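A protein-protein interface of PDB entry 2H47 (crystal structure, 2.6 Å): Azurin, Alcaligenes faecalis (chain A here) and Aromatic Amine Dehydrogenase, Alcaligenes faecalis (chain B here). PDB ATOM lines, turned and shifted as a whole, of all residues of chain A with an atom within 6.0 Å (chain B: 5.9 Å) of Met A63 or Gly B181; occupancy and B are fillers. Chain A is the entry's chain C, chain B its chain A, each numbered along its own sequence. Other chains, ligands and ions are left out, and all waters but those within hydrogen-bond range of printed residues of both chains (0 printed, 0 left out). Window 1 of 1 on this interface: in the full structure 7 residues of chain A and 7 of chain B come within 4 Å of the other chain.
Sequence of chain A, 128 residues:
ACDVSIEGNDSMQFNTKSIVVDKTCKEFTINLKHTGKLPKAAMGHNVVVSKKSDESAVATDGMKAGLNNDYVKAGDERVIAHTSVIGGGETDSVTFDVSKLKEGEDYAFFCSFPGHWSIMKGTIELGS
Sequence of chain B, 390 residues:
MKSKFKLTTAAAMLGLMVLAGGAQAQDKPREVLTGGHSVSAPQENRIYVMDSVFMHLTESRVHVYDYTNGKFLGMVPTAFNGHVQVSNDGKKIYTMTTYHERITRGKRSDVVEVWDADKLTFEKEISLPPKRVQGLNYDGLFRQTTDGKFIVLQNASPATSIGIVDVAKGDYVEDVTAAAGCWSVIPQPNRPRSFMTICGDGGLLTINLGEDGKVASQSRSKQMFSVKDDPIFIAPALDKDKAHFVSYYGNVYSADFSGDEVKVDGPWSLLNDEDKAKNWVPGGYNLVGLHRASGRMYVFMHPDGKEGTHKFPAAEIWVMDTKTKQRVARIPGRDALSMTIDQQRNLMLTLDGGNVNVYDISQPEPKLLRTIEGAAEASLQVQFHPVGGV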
ATOM      1  N   VAL A  58     -14.727  30.113 -29.222  1.00  0.00           N
ATOM      2  CA  VAL A  58     -15.958  29.331 -29.357  1.00  0.00           C
ATOM      3  C   VAL A  58     -16.254  28.521 -28.098  1.00  0.00           C
ATOM      4  O   VAL A  58     -17.395  28.454 -27.646  1.00  0.00           O
ATOM      5  CB  VAL A  58     -15.883  28.354 -30.562  1.00  0.00           C
ATOM      6  CG1 VAL A  58     -17.072  27.404 -30.544  1.00  0.00           C
ATOM      7  CG2 VAL A  58     -15.873  29.139 -31.866  1.00  0.00           C
ATOM      8  N   ALA A  59     -15.218  27.903 -27.541  1.00  0.00           N
ATOM      9  CA  ALA A  59     -15.348  27.093 -26.334  1.00  0.00           C
ATOM     10  C   ALA A  59     -15.847  27.908 -25.138  1.00  0.00           C
ATOM     11  O   ALA A  59     -16.590  27.399 -24.296  1.00  0.00           O
ATOM     12  CB  ALA A  59     -14.003  26.452 -26.001  1.00  0.00           C
ATOM     13  N   THR A  60     -15.438  29.167 -25.073  1.00  0.00           N
ATOM     14  CA  THR A  60     -15.824  30.053 -23.975  1.00  0.00           C
ATOM     15  C   THR A  60     -17.259  30.555 -24.072  1.00  0.00           C
ATOM     16  O   THR A  60     -17.964  30.610 -23.065  1.00  0.00           O
ATOM     17  CB  THR A  60     -14.887  31.277 -23.888  1.00  0.00           C
ATOM     18  OG1 THR A  60     -13.560  30.840 -23.576  1.00  0.00           O
ATOM     19  CG2 THR A  60     -15.362  32.243 -22.810  1.00  0.00           C
ATOM     20  N   ASP A  61     -17.685  30.929 -25.275  1.00  0.00           N
ATOM     21  CA  ASP A  61     -19.044  31.426 -25.482  1.00  0.00           C
ATOM     22  C   ASP A  61     -20.065  30.306 -25.314  1.00  0.00           C
ATOM     23  O   ASP A  61     -21.178  30.536 -24.834  1.00  0.00           O
ATOM     24  CB  ASP A  61     -19.181  32.052 -26.879  1.00  0.00           C
ATOM     25  CG  ASP A  61     -18.621  33.467 -26.951  1.00  0.00           C
ATOM     26  OD1 ASP A  61     -18.476  33.989 -28.077  1.00  0.00           O
ATOM     27  OD2 ASP A  61     -18.335  34.065 -25.887  1.00  0.00           O
ATOM     28  N   GLY A  62     -19.674  29.095 -25.706  1.00  0.00           N
ATOM     29  CA  GLY A  62     -20.560  27.948 -25.597  1.00  0.00           C
ATOM     30  C   GLY A  62     -20.759  27.536 -24.156  1.00  0.00           C
ATOM     31  O   GLY A  62     -21.805  27.009 -23.781  1.00  0.00           O
ATOM     32  N   MET A  63     -19.739  27.773 -23.346  1.00  0.00           N
ATOM     33  CA  MET A  63     -19.794  27.447 -21.933  1.00  0.00           C
ATOM     34  C   MET A  63     -20.911  28.240 -21.272  1.00  0.00           C
ATOM     35  O   MET A  63     -21.553  27.764 -20.335  1.00  0.00           O
ATOM     36  CB  MET A  63     -18.450  27.766 -21.275  1.00  0.00           C
ATOM     37  CG  MET A  63     -18.485  27.876 -19.762  1.00  0.00           C
ATOM     38  SD  MET A  63     -18.266  29.583 -19.207  1.00  0.00           S
ATOM     39  CE  MET A  63     -19.725  29.803 -18.158  1.00  0.00           C
ATOM     40  N   LYS A  64     -21.147  29.454 -21.762  1.00  0.00           N
ATOM     41  CA  LYS A  64     -22.204  30.289 -21.202  1.00  0.00           C
ATOM     42  C   LYS A  64     -23.560  29.855 -21.769  1.00  0.00           C
ATOM     43  O   LYS A  64     -24.610  30.240 -21.258  1.00  0.00           O
ATOM     44  CB  LYS A  64     -21.951  31.770 -21.518  1.00  0.00           C
ATOM     45  CG  LYS A  64     -20.568  32.280 -21.127  1.00  0.00           C
ATOM     46  CD  LYS A  64     -20.557  33.801 -21.035  1.00  0.00           C
ATOM     47  CE  LYS A  64     -19.152  34.381 -21.148  1.00  0.00           C
ATOM     48  NZ  LYS A  64     -18.630  34.393 -22.551  1.00  0.00           N
ATOM     49  N   ALA A  65     -23.521  29.035 -22.816  1.00  0.00           N
ATOM     50  CA  ALA A  65     -24.731  28.544 -23.464  1.00  0.00           C
ATOM     51  C   ALA A  65     -25.453  27.507 -22.614  1.00  0.00           C
ATOM     52  O   ALA A  65     -26.679  27.521 -22.507  1.00  0.00           O
ATOM     53  CB  ALA A  65     -24.387  27.952 -24.829  1.00  0.00           C
ATOM     54  N   GLY A  66     -24.692  26.596 -22.023  1.00  0.00           N
ATOM     55  CA  GLY A  66     -25.300  25.577 -21.190  1.00  0.00           C
ATOM     56  C   GLY A  66     -25.579  24.270 -21.904  1.00  0.00           C
ATOM     57  O   GLY A  66     -25.720  24.235 -23.126  1.00  0.00           O
ATOM     58  N   TYR A  71     -23.789  23.254 -25.128  1.00  0.00           N
ATOM     59  CA  TYR A  71     -22.576  24.026 -24.888  1.00  0.00           C
ATOM     60  C   TYR A  71     -21.975  24.683 -26.112  1.00  0.00           C
ATOM     61  O   TYR A  71     -20.758  24.724 -26.283  1.00  0.00           O
ATOM     62  CB  TYR A  71     -21.533  23.158 -24.188  1.00  0.00           C
ATOM     63  CG  TYR A  71     -21.803  23.044 -22.715  1.00  0.00           C
ATOM     64  CD1 TYR A  71     -21.851  24.183 -21.912  1.00  0.00           C
ATOM     65  CD2 TYR A  71     -22.035  21.808 -22.122  1.00  0.00           C
ATOM     66  CE1 TYR A  71     -22.124  24.094 -20.559  1.00  0.00           C
ATOM     67  CE2 TYR A  71     -22.307  21.709 -20.765  1.00  0.00           C
ATOM     68  CZ  TYR A  71     -22.348  22.855 -19.990  1.00  0.00           C
ATOM     69  OH  TYR A  71     -22.602  22.762 -18.644  1.00  0.00           O
ATOM     70  N   VAL A  72     -22.848  25.200 -26.963  1.00  0.00           N
ATOM     71  CA  VAL A  72     -22.435  25.899 -28.166  1.00  0.00           C
ATOM     72  C   VAL A  72     -23.356  27.105 -28.212  1.00  0.00           C
ATOM     73  O   VAL A  72     -24.539  26.991 -27.893  1.00  0.00           O
ATOM     74  CB  VAL A  72     -22.650  25.040 -29.425  1.00  0.00           C
ATOM     75  CG1 VAL A  72     -22.187  25.801 -30.658  1.00  0.00           C
ATOM     76  CG2 VAL A  72     -21.887  23.737 -29.297  1.00  0.00           C
ATOM     77  N   SER A 112     -16.658  21.635 -26.432  1.00  0.00           N
ATOM     78  CA  SER A 112     -16.963  22.891 -25.761  1.00  0.00           C
ATOM     79  C   SER A 112     -17.500  22.677 -24.341  1.00  0.00           C
ATOM     80  O   SER A 112     -17.847  23.639 -23.649  1.00  0.00           O
ATOM     81  CB  SER A 112     -17.964  23.695 -26.597  1.00  0.00           C
ATOM     82  OG  SER A 112     -19.080  22.897 -26.960  1.00  0.00           O
ATOM     83  N   PRO A 114     -17.486  22.725 -20.806  1.00  0.00           N
ATOM     84  CA  PRO A 114     -16.633  23.465 -19.873  1.00  0.00           C
ATOM     85  C   PRO A 114     -15.313  22.821 -19.438  1.00  0.00           C
ATOM     86  O   PRO A 114     -15.296  21.872 -18.644  1.00  0.00           O
ATOM     87  CB  PRO A 114     -17.574  23.743 -18.707  1.00  0.00           C
ATOM     88  CG  PRO A 114     -18.839  24.043 -19.418  1.00  0.00           C
ATOM     89  CD  PRO A 114     -18.908  22.943 -20.474  1.00  0.00           C
ATOM     90  N   THR B 160     -19.448  22.190 -12.718  1.00  0.00           N
ATOM     91  CA  THR B 160     -19.783  23.050 -11.584  1.00  0.00           C
ATOM     92  C   THR B 160     -21.195  23.623 -11.590  1.00  0.00           C
ATOM     93  O   THR B 160     -21.824  23.783 -12.637  1.00  0.00           O
ATOM     94  CB  THR B 160     -18.808  24.243 -11.473  1.00  0.00           C
ATOM     95  OG1 THR B 160     -19.022  25.147 -12.565  1.00  0.00           O
ATOM     96  CG2 THR B 160     -17.371  23.757 -11.489  1.00  0.00           C
ATOM     97  N   ALA B 178     -26.760  27.801 -13.955  1.00  0.00           N
ATOM     98  CA  ALA B 178     -26.290  28.863 -14.835  1.00  0.00           C
ATOM     99  C   ALA B 178     -24.853  29.240 -14.447  1.00  0.00           C
ATOM    100  O   ALA B 178     -24.127  29.875 -15.217  1.00  0.00           O
ATOM    101  CB  ALA B 178     -27.193  30.072 -14.721  1.00  0.00           C
ATOM    102  N   ALA B 179     -24.445  28.845 -13.247  1.00  0.00           N
ATOM    103  CA  ALA B 179     -23.099  29.140 -12.782  1.00  0.00           C
ATOM    104  C   ALA B 179     -22.082  28.131 -13.321  1.00  0.00           C
ATOM    105  O   ALA B 179     -20.906  28.174 -12.963  1.00  0.00           O
ATOM    106  CB  ALA B 179     -23.064  29.154 -11.264  1.00  0.00           C
ATOM    107  N   ALA B 180     -22.545  27.222 -14.174  1.00  0.00           N
ATOM    108  CA  ALA B 180     -21.677  26.213 -14.770  1.00  0.00           C
ATOM    109  C   ALA B 180     -20.542  26.910 -15.516  1.00  0.00           C
ATOM    110  O   ALA B 180     -20.776  27.839 -16.287  1.00  0.00           O
ATOM    111  CB  ALA B 180     -22.476  25.336 -15.730  1.00  0.00           C
ATOM    112  N   GLY B 181     -19.314  26.455 -15.288  1.00  0.00           N
ATOM    113  CA  GLY B 181     -18.180  27.064 -15.944  1.00  0.00           C
ATOM    114  C   GLY B 181     -17.665  28.210 -15.090  1.00  0.00           C
ATOM    115  O   GLY B 181     -16.804  28.983 -15.525  1.00  0.00           O
ATOM    116  N   CYS B 182     -18.212  28.331 -13.880  1.00  0.00           N
ATOM    117  CA  CYS B 182     -17.798  29.363 -12.932  1.00  0.00           C
ATOM    118  C   CYS B 182     -17.300  28.717 -11.631  1.00  0.00           C
ATOM    119  O   CYS B 182     -17.292  27.493 -11.513  1.00  0.00           O
ATOM    120  CB  CYS B 182     -18.975  30.311 -12.661  1.00  0.00           C
ATOM    121  SG  CYS B 182     -19.817  31.018 -14.128  1.00  0.00           S
ATOM    122  N   TRP B 183     -16.900  29.534 -10.660  1.00  0.00           N
ATOM    123  CA  TRP B 183     -16.404  28.996  -9.392  1.00  0.00           C
ATOM    124  C   TRP B 183     -16.467  29.999  -8.232  1.00  0.00           C
ATOM    125  O   TRP B 183     -16.302  31.200  -8.429  1.00  0.00           O
ATOM    126  CB  TRP B 183     -14.959  28.497  -9.572  1.00  0.00           C
ATOM    127  CG  TRP B 183     -14.466  27.631  -8.442  1.00  0.00           C
ATOM    128  CD1 TRP B 183     -13.487  27.933  -7.543  1.00  0.00           C
ATOM    129  CD2 TRP B 183     -14.952  26.329  -8.085  1.00  0.00           C
ATOM    130  NE1 TRP B 183     -13.329  26.901  -6.646  1.00  0.00           N
ATOM    131  CE2 TRP B 183     -14.216  25.906  -6.955  1.00  0.00           C
ATOM    132  CE3 TRP B 183     -15.937  25.479  -8.608  1.00  0.00           C
ATOM    133  CZ2 TRP B 183     -14.437  24.669  -6.341  1.00  0.00           C
ATOM    134  CZ3 TRP B 183     -16.152  24.252  -7.995  1.00  0.00           C
ATOM    135  CH2 TRP B 183     -15.405  23.861  -6.874  1.00  0.00           C
ATOM    136  N   ILE B 198     -17.119  33.884 -10.095  1.00  0.00           N
ATOM    137  CA  ILE B 198     -16.117  34.143 -11.125  1.00  0.00           C
ATOM    138  C   ILE B 198     -16.259  33.083 -12.208  1.00  0.00           C
ATOM    139  O   ILE B 198     -16.422  31.905 -11.895  1.00  0.00           O
ATOM    140  CB  ILE B 198     -14.687  34.088 -10.536  1.00  0.00           C
ATOM    141  CG1 ILE B 198     -14.608  34.982  -9.299  1.00  0.00           C
ATOM    142  CG2 ILE B 198     -13.672  34.575 -11.561  1.00  0.00           C
ATOM    143  CD1 ILE B 198     -13.251  34.965  -8.616  1.00  0.00           C
ATOM    144  N   CYS B 199     -16.207  33.492 -13.475  1.00  0.00           N
ATOM    145  CA  CYS B 199     -16.349  32.540 -14.574  1.00  0.00           C
ATOM    146  C   CYS B 199     -15.169  32.476 -15.538  1.00  0.00           C
ATOM    147  O   CYS B 199     -14.372  33.409 -15.627  1.00  0.00           O
ATOM    148  CB  CYS B 199     -17.646  32.836 -15.330  1.00  0.00           C
ATOM    149  SG  CYS B 199     -19.116  32.936 -14.248  1.00  0.00           S
ATOM    150  N   GLY B 200     -15.079  31.368 -16.268  1.00  0.00           N
ATOM    151  CA  GLY B 200     -13.993  31.181 -17.209  1.00  0.00           C
ATOM    152  C   GLY B 200     -13.812  32.263 -18.262  1.00  0.00           C
ATOM    153  O   GLY B 200     -12.805  32.278 -18.973  1.00  0.00           O
ATOM    154  N   ASP B 201     -14.775  33.173 -18.374  1.00  0.00           N
ATOM    155  CA  ASP B 201     -14.690  34.240 -19.364  1.00  0.00           C
ATOM    156  C   ASP B 201     -14.070  35.497 -18.766  1.00  0.00           C
ATOM    157  O   ASP B 201     -13.893  36.494 -19.462  1.00  0.00           O
ATOM    158  CB  ASP B 201     -16.077  34.576 -19.884  1.00  0.00           C
ATOM    159  CG  ASP B 201     -16.898  35.331 -18.867  1.00  0.00           C
ATOM    160  OD1 ASP B 201     -16.692  35.090 -17.653  1.00  0.00           O
ATOM    161  OD2 ASP B 201     -17.750  36.154 -19.277  1.00  0.00           O
ATOM    162  N   ARG B 220     -24.728  39.061 -16.307  1.00  0.00           N
ATOM    163  CA  ARG B 220     -23.302  38.852 -16.520  1.00  0.00           C
ATOM    164  C   ARG B 220     -22.610  40.188 -16.706  1.00  0.00           C
ATOM    165  O   ARG B 220     -23.129  41.075 -17.384  1.00  0.00           O
ATOM    166  CB  ARG B 220     -23.046  37.984 -17.760  1.00  0.00           C
ATOM    167  CG  ARG B 220     -22.945  36.494 -17.482  1.00  0.00           C
ATOM    168  CD  ARG B 220     -21.814  35.860 -18.285  1.00  0.00           C
ATOM    169  NE  ARG B 220     -21.389  34.584 -17.711  1.00  0.00           N
ATOM    170  CZ  ARG B 220     -22.094  33.461 -17.781  1.00  0.00           C
ATOM    171  NH1 ARG B 220     -23.260  33.456 -18.410  1.00  0.00           N
ATOM    172  NH2 ARG B 220     -21.638  32.348 -17.223  1.00  0.00           N
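Printed residues of chain A that touch a printed residue of chain B: Thr A60, Met A63, Lys A64 and Tyr A71. Hydrophobic or aromatic side chains of chain A within 4 Å of the printed part of chain B: Met A63 and Tyr A71. Among the printed residues, 7 pairs touch across the chains.
Among the printed residues, pairs that only touch across the chains: Thr A60 with Asp B201 (3.8 Å), Met A63 with Ala B180 (2.9 Å), Met A63 with Gly B181 (3.8 Å), Met A63 with Arg B220 (3.3 Å), Lys A64 with Arg B220 (3.5 Å) and Tyr A71 with Ala B180 (3.9 Å).
Met A63 touches just these residues of chain B: Ala B180 (2.9 Å), Gly B181 (3.8 Å) and Arg B220 (3.3 Å). Of chain A, only Met A63 (3.8 Å) comes within 4 Å of Gly B181. Of the printed residues of chain B, Tyr A71 touches Ala B180 (3.9 Å). Of the printed residues of chain B, Thr A60 touches Asp B201. Of the printed residues of chain A, Asp B201 touches Thr A60 (3.8 Å) and Lys A64 (2.9 Å). Of the printed residues of chain A, Ala B180 touches Met A63 and Tyr A71. Val A72 touches none of the printed residues of chain B. The nearest residue of chain B that does not touch Met A63 is Cys B182 (4.2 Å). The nearest residue of chain A that does not touch Gly B181 is Pro A114 (4.4 Å).
The side-chain carboxylate of Asp B201 lies within salt-bridge range of the side-chain amino group of Lys A64 (3.8 Å).
N of Gly B181 is in hydrogen-bond range of OG1 of Thr B160 (3.0 Å). The backbone carbonyl oxygen (O) of Gly B181 sits at hydrogen-bond distance from the backbone NH (N) of Gly B200 (3.0 Å). The side-chain carboxylate of Asp A61 is in salt-bridge range of the side-chain amino group of Lys A64, at 3.4 Å. N of Tyr A71 is in hydrogen-bond range of O of Gly A66 (2.9 Å). The side-chain hydroxyl (OG) of Ser A112 lies within hydrogen-bond range of the backbone carbonyl oxygen (O) of Tyr A71. SG of Cys B182 is disulfide-bonded to SG of Cys B199 (2.0 Å).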
